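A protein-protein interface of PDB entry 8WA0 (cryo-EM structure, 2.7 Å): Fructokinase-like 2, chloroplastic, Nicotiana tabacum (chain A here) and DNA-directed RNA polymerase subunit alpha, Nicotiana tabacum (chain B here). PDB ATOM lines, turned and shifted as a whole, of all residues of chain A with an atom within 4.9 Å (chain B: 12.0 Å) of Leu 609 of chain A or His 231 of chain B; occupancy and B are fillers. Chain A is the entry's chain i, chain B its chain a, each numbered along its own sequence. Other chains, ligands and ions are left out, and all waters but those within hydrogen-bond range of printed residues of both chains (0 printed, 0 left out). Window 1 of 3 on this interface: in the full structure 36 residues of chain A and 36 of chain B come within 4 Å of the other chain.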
ATOM      1  N   VAL A 605       7.564 -20.632   8.494  1.00  0.00           N
ATOM      2  CA  VAL A 605       6.881 -19.397   8.878  1.00  0.00           C
ATOM      3  C   VAL A 605       6.153 -19.592  10.204  1.00  0.00           C
ATOM      4  O   VAL A 605       6.303 -18.782  11.117  1.00  0.00           O
ATOM      5  CB  VAL A 605       5.922 -18.901   7.777  1.00  0.00           C
ATOM      6  CG1 VAL A 605       5.028 -17.784   8.290  1.00  0.00           C
ATOM      7  CG2 VAL A 605       6.709 -18.431   6.565  1.00  0.00           C
ATOM      8  N   ASP A 606       5.384 -20.668  10.331  1.00  0.00           N
ATOM      9  CA  ASP A 606       4.712 -20.967  11.588  1.00  0.00           C
ATOM     10  C   ASP A 606       5.532 -21.182  12.830  1.00  0.00           C
ATOM     11  O   ASP A 606       5.166 -20.672  13.864  1.00  0.00           O
ATOM     12  CB  ASP A 606       3.757 -22.072  11.373  1.00  0.00           C
ATOM     13  CG  ASP A 606       2.617 -21.680  10.471  1.00  0.00           C
ATOM     14  OD1 ASP A 606       2.461 -20.471  10.201  1.00  0.00           O
ATOM     15  OD2 ASP A 606       1.870 -22.578  10.032  1.00  0.00           O
ATOM     16  N   GLN A 607       6.631 -21.882  12.780  1.00  0.00           N
ATOM     17  CA  GLN A 607       7.461 -21.996  13.919  1.00  0.00           C
ATOM     18  C   GLN A 607       8.030 -20.668  14.309  1.00  0.00           C
ATOM     19  O   GLN A 607       8.104 -20.374  15.489  1.00  0.00           O
ATOM     20  CB  GLN A 607       8.494 -23.092  13.751  1.00  0.00           C
ATOM     21  CG  GLN A 607       9.129 -23.598  15.006  1.00  0.00           C
ATOM     22  CD  GLN A 607       8.257 -24.590  15.693  1.00  0.00           C
ATOM     23  OE1 GLN A 607       8.462 -24.904  16.848  1.00  0.00           O
ATOM     24  NE2 GLN A 607       7.274 -25.097  14.987  1.00  0.00           N
ATOM     25  N   TRP A 608       8.413 -19.825  13.354  1.00  0.00           N
ATOM     26  CA  TRP A 608       8.938 -18.515  13.632  1.00  0.00           C
ATOM     27  C   TRP A 608       7.952 -17.609  14.278  1.00  0.00           C
ATOM     28  O   TRP A 608       8.282 -16.881  15.200  1.00  0.00           O
ATOM     29  CB  TRP A 608       9.274 -17.853  12.362  1.00  0.00           C
ATOM     30  CG  TRP A 608      10.633 -17.926  11.800  1.00  0.00           C
ATOM     31  CD1 TRP A 608      11.135 -18.913  11.015  1.00  0.00           C
ATOM     32  CD2 TRP A 608      11.633 -16.909  11.852  1.00  0.00           C
ATOM     33  NE1 TRP A 608      12.408 -18.599  10.614  1.00  0.00           N
ATOM     34  CE2 TRP A 608      12.736 -17.370  11.112  1.00  0.00           C
ATOM     35  CE3 TRP A 608      11.714 -15.669  12.470  1.00  0.00           C
ATOM     36  CZ2 TRP A 608      13.900 -16.643  10.986  1.00  0.00           C
ATOM     37  CZ3 TRP A 608      12.861 -14.953  12.338  1.00  0.00           C
ATOM     38  CH2 TRP A 608      13.944 -15.436  11.604  1.00  0.00           C
ATOM     39  N   LEU A 609       6.734 -17.620  13.776  1.00  0.00           N
ATOM     40  CA  LEU A 609       5.722 -16.736  14.301  1.00  0.00           C
ATOM     41  C   LEU A 609       5.434 -17.091  15.726  1.00  0.00           C
ATOM     42  O   LEU A 609       5.223 -16.218  16.542  1.00  0.00           O
ATOM     43  CB  LEU A 609       4.448 -16.810  13.479  1.00  0.00           C
ATOM     44  CG  LEU A 609       4.380 -16.216  12.078  1.00  0.00           C
ATOM     45  CD1 LEU A 609       3.075 -16.608  11.415  1.00  0.00           C
ATOM     46  CD2 LEU A 609       4.507 -14.711  12.125  1.00  0.00           C
ATOM     47  N   GLN A 610       5.420 -18.370  16.042  1.00  0.00           N
ATOM     48  CA  GLN A 610       5.078 -18.775  17.384  1.00  0.00           C
ATOM     49  C   GLN A 610       6.069 -18.265  18.376  1.00  0.00           C
ATOM     50  O   GLN A 610       5.698 -17.795  19.431  1.00  0.00           O
ATOM     51  CB  GLN A 610       4.984 -20.273  17.508  1.00  0.00           C
ATOM     52  CG  GLN A 610       4.310 -20.717  18.793  1.00  0.00           C
ATOM     53  CD  GLN A 610       4.167 -22.217  18.893  1.00  0.00           C
ATOM     54  OE1 GLN A 610       4.529 -22.946  17.978  1.00  0.00           O
ATOM     55  NE2 GLN A 610       3.640 -22.685  20.012  1.00  0.00           N
ATOM     56  N   ALA A 611       7.336 -18.319  18.038  1.00  0.00           N
ATOM     57  CA  ALA A 611       8.358 -17.901  18.966  1.00  0.00           C
ATOM     58  C   ALA A 611       8.181 -16.466  19.302  1.00  0.00           C
ATOM     59  O   ALA A 611       8.348 -16.061  20.436  1.00  0.00           O
ATOM     60  CB  ALA A 611       9.709 -18.086  18.341  1.00  0.00           C
ATOM     61  N   ARG A 612       7.882 -15.671  18.301  1.00  0.00           N
ATOM     62  CA  ARG A 612       7.674 -14.271  18.527  1.00  0.00           C
ATOM     63  C   ARG A 612       6.451 -14.007  19.378  1.00  0.00           C
ATOM     64  O   ARG A 612       6.498 -13.174  20.269  1.00  0.00           O
ATOM     65  CB  ARG A 612       7.589 -13.549  17.197  1.00  0.00           C
ATOM     66  CG  ARG A 612       8.511 -12.355  17.095  1.00  0.00           C
ATOM     67  CD  ARG A 612       9.895 -12.706  17.601  1.00  0.00           C
ATOM     68  NE  ARG A 612      10.728 -13.315  16.576  1.00  0.00           N
ATOM     69  CZ  ARG A 612      11.937 -13.810  16.810  1.00  0.00           C
ATOM     70  NH1 ARG A 612      12.640 -14.343  15.826  1.00  0.00           N
ATOM     71  NH2 ARG A 612      12.438 -13.784  18.034  1.00  0.00           N
ATOM     72  N   ARG A 613       5.373 -14.737  19.146  1.00  0.00           N
ATOM     73  CA  ARG A 613       4.162 -14.559  19.931  1.00  0.00           C
ATOM     74  C   ARG A 613       4.338 -14.998  21.364  1.00  0.00           C
ATOM     75  O   ARG A 613       4.185 -14.208  22.272  1.00  0.00           O
ATOM     76  CB  ARG A 613       3.014 -15.313  19.301  1.00  0.00           C
ATOM     77  CG  ARG A 613       1.674 -15.101  19.969  1.00  0.00           C
ATOM     78  CD  ARG A 613       0.635 -15.925  19.242  1.00  0.00           C
ATOM     79  NE  ARG A 613       1.150 -17.260  18.968  1.00  0.00           N
ATOM     80  CZ  ARG A 613       0.509 -18.178  18.257  1.00  0.00           C
ATOM     81  NH1 ARG A 613       1.057 -19.368  18.059  1.00  0.00           N
ATOM     82  NH2 ARG A 613      -0.680 -17.905  17.740  1.00  0.00           N
ATOM     83  N   ARG B 220      18.409 -13.186   8.645  1.00  0.00           N
ATOM     84  CA  ARG B 220      17.515 -13.321   9.744  1.00  0.00           C
ATOM     85  C   ARG B 220      16.879 -12.042  10.153  1.00  0.00           C
ATOM     86  O   ARG B 220      15.722 -12.014  10.461  1.00  0.00           O
ATOM     87  CB  ARG B 220      18.256 -13.887  10.911  1.00  0.00           C
ATOM     88  CG  ARG B 220      18.725 -15.300  10.709  1.00  0.00           C
ATOM     89  CD  ARG B 220      19.568 -15.780  11.870  1.00  0.00           C
ATOM     90  NE  ARG B 220      20.314 -16.965  11.470  1.00  0.00           N
ATOM     91  CZ  ARG B 220      19.891 -18.213  11.632  1.00  0.00           C
ATOM     92  NH1 ARG B 220      18.734 -18.463  12.225  1.00  0.00           N
ATOM     93  NH2 ARG B 220      20.643 -19.217  11.212  1.00  0.00           N
ATOM     94  N   LEU B 222      16.259  -9.470   8.275  1.00  0.00           N
ATOM     95  CA  LEU B 222      15.276  -9.144   7.265  1.00  0.00           C
ATOM     96  C   LEU B 222      13.986  -9.903   7.369  1.00  0.00           C
ATOM     97  O   LEU B 222      12.958  -9.322   7.227  1.00  0.00           O
ATOM     98  CB  LEU B 222      15.873  -9.293   5.880  1.00  0.00           C
ATOM     99  CG  LEU B 222      16.774  -8.210   5.300  1.00  0.00           C
ATOM    100  CD1 LEU B 222      17.395  -8.706   4.015  1.00  0.00           C
ATOM    101  CD2 LEU B 222      16.006  -6.932   5.054  1.00  0.00           C
ATOM    102  N   ILE B 223      14.006 -11.184   7.657  1.00  0.00           N
ATOM    103  CA  ILE B 223      12.801 -11.979   7.858  1.00  0.00           C
ATOM    104  C   ILE B 223      12.028 -11.476   9.063  1.00  0.00           C
ATOM    105  O   ILE B 223      10.833 -11.420   9.031  1.00  0.00           O
ATOM    106  CB  ILE B 223      13.094 -13.493   7.871  1.00  0.00           C
ATOM    107  CG1 ILE B 223      13.622 -13.931   6.512  1.00  0.00           C
ATOM    108  CG2 ILE B 223      11.872 -14.296   8.246  1.00  0.00           C
ATOM    109  CD1 ILE B 223      14.487 -15.162   6.553  1.00  0.00           C
ATOM    110  N   ASP B 224      12.693 -11.048  10.106  1.00  0.00           N
ATOM    111  CA  ASP B 224      12.043 -10.508  11.276  1.00  0.00           C
ATOM    112  C   ASP B 224      11.396  -9.207  11.069  1.00  0.00           C
ATOM    113  O   ASP B 224      10.700  -8.762  11.937  1.00  0.00           O
ATOM    114  CB  ASP B 224      13.006 -10.362  12.391  1.00  0.00           C
ATOM    115  CG  ASP B 224      13.081 -11.580  13.249  1.00  0.00           C
ATOM    116  OD1 ASP B 224      12.035 -12.207  13.463  1.00  0.00           O
ATOM    117  OD2 ASP B 224      14.179 -11.911  13.727  1.00  0.00           O
ATOM    118  N   LEU B 225      11.680  -8.534   9.979  1.00  0.00           N
ATOM    119  CA  LEU B 225      11.041  -7.286   9.645  1.00  0.00           C
ATOM    120  C   LEU B 225       9.891  -7.460   8.692  1.00  0.00           C
ATOM    121  O   LEU B 225       9.123  -6.556   8.506  1.00  0.00           O
ATOM    122  CB  LEU B 225      12.047  -6.357   9.016  1.00  0.00           C
ATOM    123  CG  LEU B 225      13.189  -5.721   9.788  1.00  0.00           C
ATOM    124  CD1 LEU B 225      14.013  -4.884   8.829  1.00  0.00           C
ATOM    125  CD2 LEU B 225      12.628  -4.864  10.900  1.00  0.00           C
ATOM    126  N   PHE B 226       9.771  -8.615   8.067  1.00  0.00           N
ATOM    127  CA  PHE B 226       8.679  -8.901   7.144  1.00  0.00           C
ATOM    128  C   PHE B 226       7.698  -9.899   7.720  1.00  0.00           C
ATOM    129  O   PHE B 226       6.624 -10.022   7.211  1.00  0.00           O
ATOM    130  CB  PHE B 226       9.208  -9.410   5.811  1.00  0.00           C
ATOM    131  CG  PHE B 226      10.152  -8.494   5.115  1.00  0.00           C
ATOM    132  CD1 PHE B 226       9.835  -7.171   4.896  1.00  0.00           C
ATOM    133  CD2 PHE B 226      11.341  -8.979   4.620  1.00  0.00           C
ATOM    134  CE1 PHE B 226      10.710  -6.336   4.238  1.00  0.00           C
ATOM    135  CE2 PHE B 226      12.222  -8.150   3.964  1.00  0.00           C
ATOM    136  CZ  PHE B 226      11.906  -6.825   3.774  1.00  0.00           C
ATOM    137  N   ILE B 227       8.048 -10.610   8.772  1.00  0.00           N
ATOM    138  CA  ILE B 227       7.180 -11.574   9.461  1.00  0.00           C
ATOM    139  C   ILE B 227       6.035 -10.942  10.215  1.00  0.00           C
ATOM    140  O   ILE B 227       4.986 -11.521  10.304  1.00  0.00           O
ATOM    141  CB  ILE B 227       8.035 -12.449  10.424  1.00  0.00           C
ATOM    142  CG1 ILE B 227       8.412 -13.815   9.833  1.00  0.00           C
ATOM    143  CG2 ILE B 227       7.487 -12.543  11.837  1.00  0.00           C
ATOM    144  CD1 ILE B 227       7.271 -14.735   9.520  1.00  0.00           C
ATOM    145  N   PRO B 228       6.218  -9.716  10.773  1.00  0.00           N
ATOM    146  CA  PRO B 228       5.048  -9.185  11.457  1.00  0.00           C
ATOM    147  C   PRO B 228       3.763  -9.157  10.683  1.00  0.00           C
ATOM    148  O   PRO B 228       2.723  -9.293  11.286  1.00  0.00           O
ATOM    149  CB  PRO B 228       5.454  -7.752  11.761  1.00  0.00           C
ATOM    150  CG  PRO B 228       6.775  -7.525  11.129  1.00  0.00           C
ATOM    151  CD  PRO B 228       7.380  -8.875  11.121  1.00  0.00           C
ATOM    152  N   PHE B 229       3.809  -8.982   9.382  1.00  0.00           N
ATOM    153  CA  PHE B 229       2.594  -8.852   8.607  1.00  0.00           C
ATOM    154  C   PHE B 229       1.743 -10.093   8.627  1.00  0.00           C
ATOM    155  O   PHE B 229       0.551 -10.013   8.428  1.00  0.00           O
ATOM    156  CB  PHE B 229       2.888  -8.449   7.180  1.00  0.00           C
ATOM    157  CG  PHE B 229       3.314  -7.023   7.026  1.00  0.00           C
ATOM    158  CD1 PHE B 229       2.428  -5.994   7.277  1.00  0.00           C
ATOM    159  CD2 PHE B 229       4.592  -6.712   6.609  1.00  0.00           C
ATOM    160  CE1 PHE B 229       2.811  -4.680   7.127  1.00  0.00           C
ATOM    161  CE2 PHE B 229       4.984  -5.399   6.458  1.00  0.00           C
ATOM    162  CZ  PHE B 229       4.090  -4.382   6.717  1.00  0.00           C
ATOM    163  N   LEU B 230       2.348 -11.250   8.807  1.00  0.00           N
ATOM    164  CA  LEU B 230       1.605 -12.492   8.786  1.00  0.00           C
ATOM    165  C   LEU B 230       0.969 -12.861  10.122  1.00  0.00           C
ATOM    166  O   LEU B 230       0.346 -13.901  10.221  1.00  0.00           O
ATOM    167  CB  LEU B 230       2.497 -13.598   8.256  1.00  0.00           C
ATOM    168  CG  LEU B 230       3.155 -13.295   6.918  1.00  0.00           C
ATOM    169  CD1 LEU B 230       4.219 -14.322   6.589  1.00  0.00           C
ATOM    170  CD2 LEU B 230       2.107 -13.238   5.826  1.00  0.00           C
ATOM    171  N   HIS B 231       1.108 -12.030  11.148  1.00  0.00           N
ATOM    172  CA  HIS B 231       0.456 -12.242  12.436  1.00  0.00           C
ATOM    173  C   HIS B 231      -0.927 -11.690  12.289  1.00  0.00           C
ATOM    174  O   HIS B 231      -1.320 -11.262  11.233  1.00  0.00           O
ATOM    175  CB  HIS B 231       1.082 -11.433  13.546  1.00  0.00           C
ATOM    176  CG  HIS B 231       2.286 -12.047  14.176  1.00  0.00           C
ATOM    177  ND1 HIS B 231       3.460 -11.352  14.350  1.00  0.00           N
ATOM    178  CD2 HIS B 231       2.493 -13.272  14.709  1.00  0.00           C
ATOM    179  CE1 HIS B 231       4.348 -12.129  14.940  1.00  0.00           C
ATOM    180  NE2 HIS B 231       3.785 -13.300  15.172  1.00  0.00           N
ATOM    181  N   MET B 232      -1.704 -11.735  13.341  1.00  0.00           N
ATOM    182  CA  MET B 232      -3.057 -11.239  13.282  1.00  0.00           C
ATOM    183  C   MET B 232      -3.135  -9.743  13.428  1.00  0.00           C
ATOM    184  O   MET B 232      -2.312  -9.157  14.110  1.00  0.00           O
ATOM    185  CB  MET B 232      -3.908 -11.908  14.334  1.00  0.00           C
ATOM    186  CG  MET B 232      -5.173 -12.535  13.762  1.00  0.00           C
ATOM    187  SD  MET B 232      -6.236 -13.336  14.979  1.00  0.00           S
ATOM    188  CE  MET B 232      -6.396 -12.018  16.174  1.00  0.00           C
ATOM    189  N   GLU B 233      -4.122  -9.113  12.818  1.00  0.00           N
ATOM    190  CA  GLU B 233      -4.212  -7.675  12.848  1.00  0.00           C
ATOM    191  C   GLU B 233      -4.481  -7.207  14.223  1.00  0.00           C
ATOM    192  O   GLU B 233      -5.117  -7.894  14.993  1.00  0.00           O
ATOM    193  CB  GLU B 233      -5.341  -7.221  11.961  1.00  0.00           C
ATOM    194  CG  GLU B 233      -5.393  -5.765  11.595  1.00  0.00           C
ATOM    195  CD  GLU B 233      -6.560  -5.500  10.683  1.00  0.00           C
ATOM    196  OE1 GLU B 233      -7.366  -6.428  10.503  1.00  0.00           O
ATOM    197  OE2 GLU B 233      -6.677  -4.387  10.145  1.00  0.00           O
ATOM    198  N   GLU B 234      -3.991  -6.035  14.560  1.00  0.00           N
ATOM    199  CA  GLU B 234      -4.290  -5.468  15.844  1.00  0.00           C
ATOM    200  C   GLU B 234      -5.570  -4.705  15.716  1.00  0.00           C
ATOM    201  O   GLU B 234      -5.706  -3.851  14.855  1.00  0.00           O
ATOM    202  CB  GLU B 234      -3.200  -4.511  16.274  1.00  0.00           C
ATOM    203  N   ASP B 235      -6.517  -4.999  16.590  1.00  0.00           N
ATOM    204  CA  ASP B 235      -7.791  -4.306  16.576  1.00  0.00           C
ATOM    205  C   ASP B 235      -8.337  -4.197  17.988  1.00  0.00           C
ATOM    206  O   ASP B 235      -8.424  -3.104  18.545  1.00  0.00           O
ATOM    207  CB  ASP B 235      -8.789  -5.064  15.722  1.00  0.00           C
ATOM    208  CG  ASP B 235      -8.910  -4.504  14.308  1.00  0.00           C
ATOM    209  OD1 ASP B 235      -8.443  -3.372  14.062  1.00  0.00           O
ATOM    210  OD2 ASP B 235      -9.488  -5.194  13.442  1.00  0.00           O
ATOM    211  N   PRO B 247       0.972  -8.544  26.151  1.00  0.00           N
ATOM    212  CA  PRO B 247       1.070  -9.464  25.022  1.00  0.00           C
ATOM    213  C   PRO B 247       1.834 -10.685  25.486  1.00  0.00           C
ATOM    214  O   PRO B 247       2.034 -10.848  26.686  1.00  0.00           O
ATOM    215  CB  PRO B 247       1.900  -8.680  24.023  1.00  0.00           C
ATOM    216  CG  PRO B 247       2.784  -7.839  24.875  1.00  0.00           C
ATOM    217  CD  PRO B 247       1.942  -7.440  26.051  1.00  0.00           C
ATOM    218  N   LEU B 248       2.198 -11.569  24.576  1.00  0.00           N
ATOM    219  CA  LEU B 248       3.014 -12.705  24.952  1.00  0.00           C
ATOM    220  C   LEU B 248       2.334 -13.571  25.985  1.00  0.00           C
ATOM    221  O   LEU B 248       2.985 -14.118  26.866  1.00  0.00           O
ATOM    222  CB  LEU B 248       4.389 -12.236  25.455  1.00  0.00           C
ATOM    223  CG  LEU B 248       5.538 -11.938  24.486  1.00  0.00           C
ATOM    224  CD1 LEU B 248       5.196 -10.881  23.450  1.00  0.00           C
ATOM    225  CD2 LEU B 248       6.763 -11.520  25.275  1.00  0.00           C
ATOM    226  N   SER B 249       1.025 -13.711  25.875  1.00  0.00           N
ATOM    227  CA  SER B 249       0.294 -14.556  26.794  1.00  0.00           C
ATOM    228  C   SER B 249      -0.467 -15.632  26.009  1.00  0.00           C
ATOM    229  O   SER B 249      -1.073 -15.315  24.992  1.00  0.00           O
ATOM    230  CB  SER B 249      -0.676 -13.730  27.625  1.00  0.00           C
ATOM    231  OG  SER B 249      -1.571 -13.012  26.798  1.00  0.00           O
ATOM    232  N   PRO B 250      -0.431 -16.912  26.449  1.00  0.00           N
ATOM    233  CA  PRO B 250      -1.221 -17.859  25.673  1.00  0.00           C
ATOM    234  C   PRO B 250      -2.692 -17.545  25.649  1.00  0.00           C
ATOM    235  O   PRO B 250      -3.311 -17.702  24.609  1.00  0.00           O
ATOM    236  CB  PRO B 250      -0.987 -19.186  26.392  1.00  0.00           C
ATOM    237  CG  PRO B 250      -0.360 -18.848  27.704  1.00  0.00           C
ATOM    238  CD  PRO B 250       0.372 -17.565  27.490  1.00  0.00           C
ATOM    239  N   THR B 252      -4.688 -14.921  25.417  1.00  0.00           N
ATOM    240  CA  THR B 252      -5.224 -13.653  25.008  1.00  0.00           C
ATOM    241  C   THR B 252      -6.658 -13.706  24.462  1.00  0.00           C
ATOM    242  O   THR B 252      -7.437 -12.814  24.746  1.00  0.00           O
ATOM    243  CB  THR B 252      -4.302 -12.989  23.986  1.00  0.00           C
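The side-chain carboxylate of Asp 224 of chain B lies within salt-bridge range of the guanidinium group of Arg 612 of chain A (3.2 Å).
Among the printed residues, merely in contact across the chains: Trp 608 of chain A with Asp 224 of chain B (3.1 Å), Arg 613 of chain A with Leu 248 of chain B (3.3 Å), Leu 609 of chain A with His 231 of chain B (3.4 Å), Leu 609 of chain A with Ile 227 of chain B (3.7 Å), Val 605 of chain A with Leu 230 of chain B (3.9 Å) and Val 605 of chain A with Ile 227 of chain B (3.98 Å).
Leu 609 of chain A touches just these residues of chain B: Ile 227 (3.7 Å) and His 231 (3.4 Å). Of chain A, only Leu 609 comes within 4 Å of His 231 of chain B. Of chain B, only Ile 227 (3.98 Å) and Leu 230 (3.9 Å) come within 4 Å of Val 605 of chain A. No residue of chain B comes within 4 Å of Asp 606 of chain A. Trp 608 of chain A touches just one residue of chain B: Asp 224 (3.1 Å). Gln 610 of chain A touches none of the printed residues of chain B. No residue of chain B comes within 4 Å of Ala 611 of chain A. Of the printed residues of chain B, Arg 613 of chain A touches Leu 248 (3.3 Å). Of the printed residues of chain A, Asp 224 of chain B touches Trp 608 and Arg 612. Printed residues of chain A within 4 Å of Leu 248 of chain B: Arg 613. Of the printed residues of chain A, Ile 227 of chain B touches Val 605 (3.98 Å) and Leu 609 (3.7 Å). Printed residues of chain A within 4 Å of Leu 230 of chain B: Val 605 (3.9 Å). Gln 607 of chain A touches none of the printed residues of chain B. Ser 249 of chain B touches none of the printed residues of chain A. The nearest residue of chain B that does not touch Leu 609 of chain A is Leu 230 of chain B (4.03 Å). The nearest residue of chain A that does not touch His 231 of chain B is Arg 612 of chain A (4.2 Å). The nearest printed residue of chain A that does not touch Leu 248 of chain B is Arg 612 of chain A (4.1 Å).
Of the 20 printed residues of chain B, 5 touch a printed residue of chain A. Printed residues of chain B that touch a printed residue of chain A: Asp 224, Ile 227, Leu 230, His 231 and Leu 248. Hydrophobic or aromatic side chains of chain B within 4 Å of the printed part of chain A: Ile 227, Leu 230, His 231 and Leu 248. Printed residues of chain A that touch a printed residue of chain B: Val 605, Trp 608, Leu 609, Arg 612 and Arg 613. Hydrophobic or aromatic side chains of chain A within 4 Å of the printed part of chain B: Val 605, Trp 608 and Leu 609. Among the printed residues, Asp or Glu carboxylates within 4 Å of a Lys or Arg side-chain nitrogen of the other chain: Arg 612 of chain A with Asp 224 of chain B (3.2 Å).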
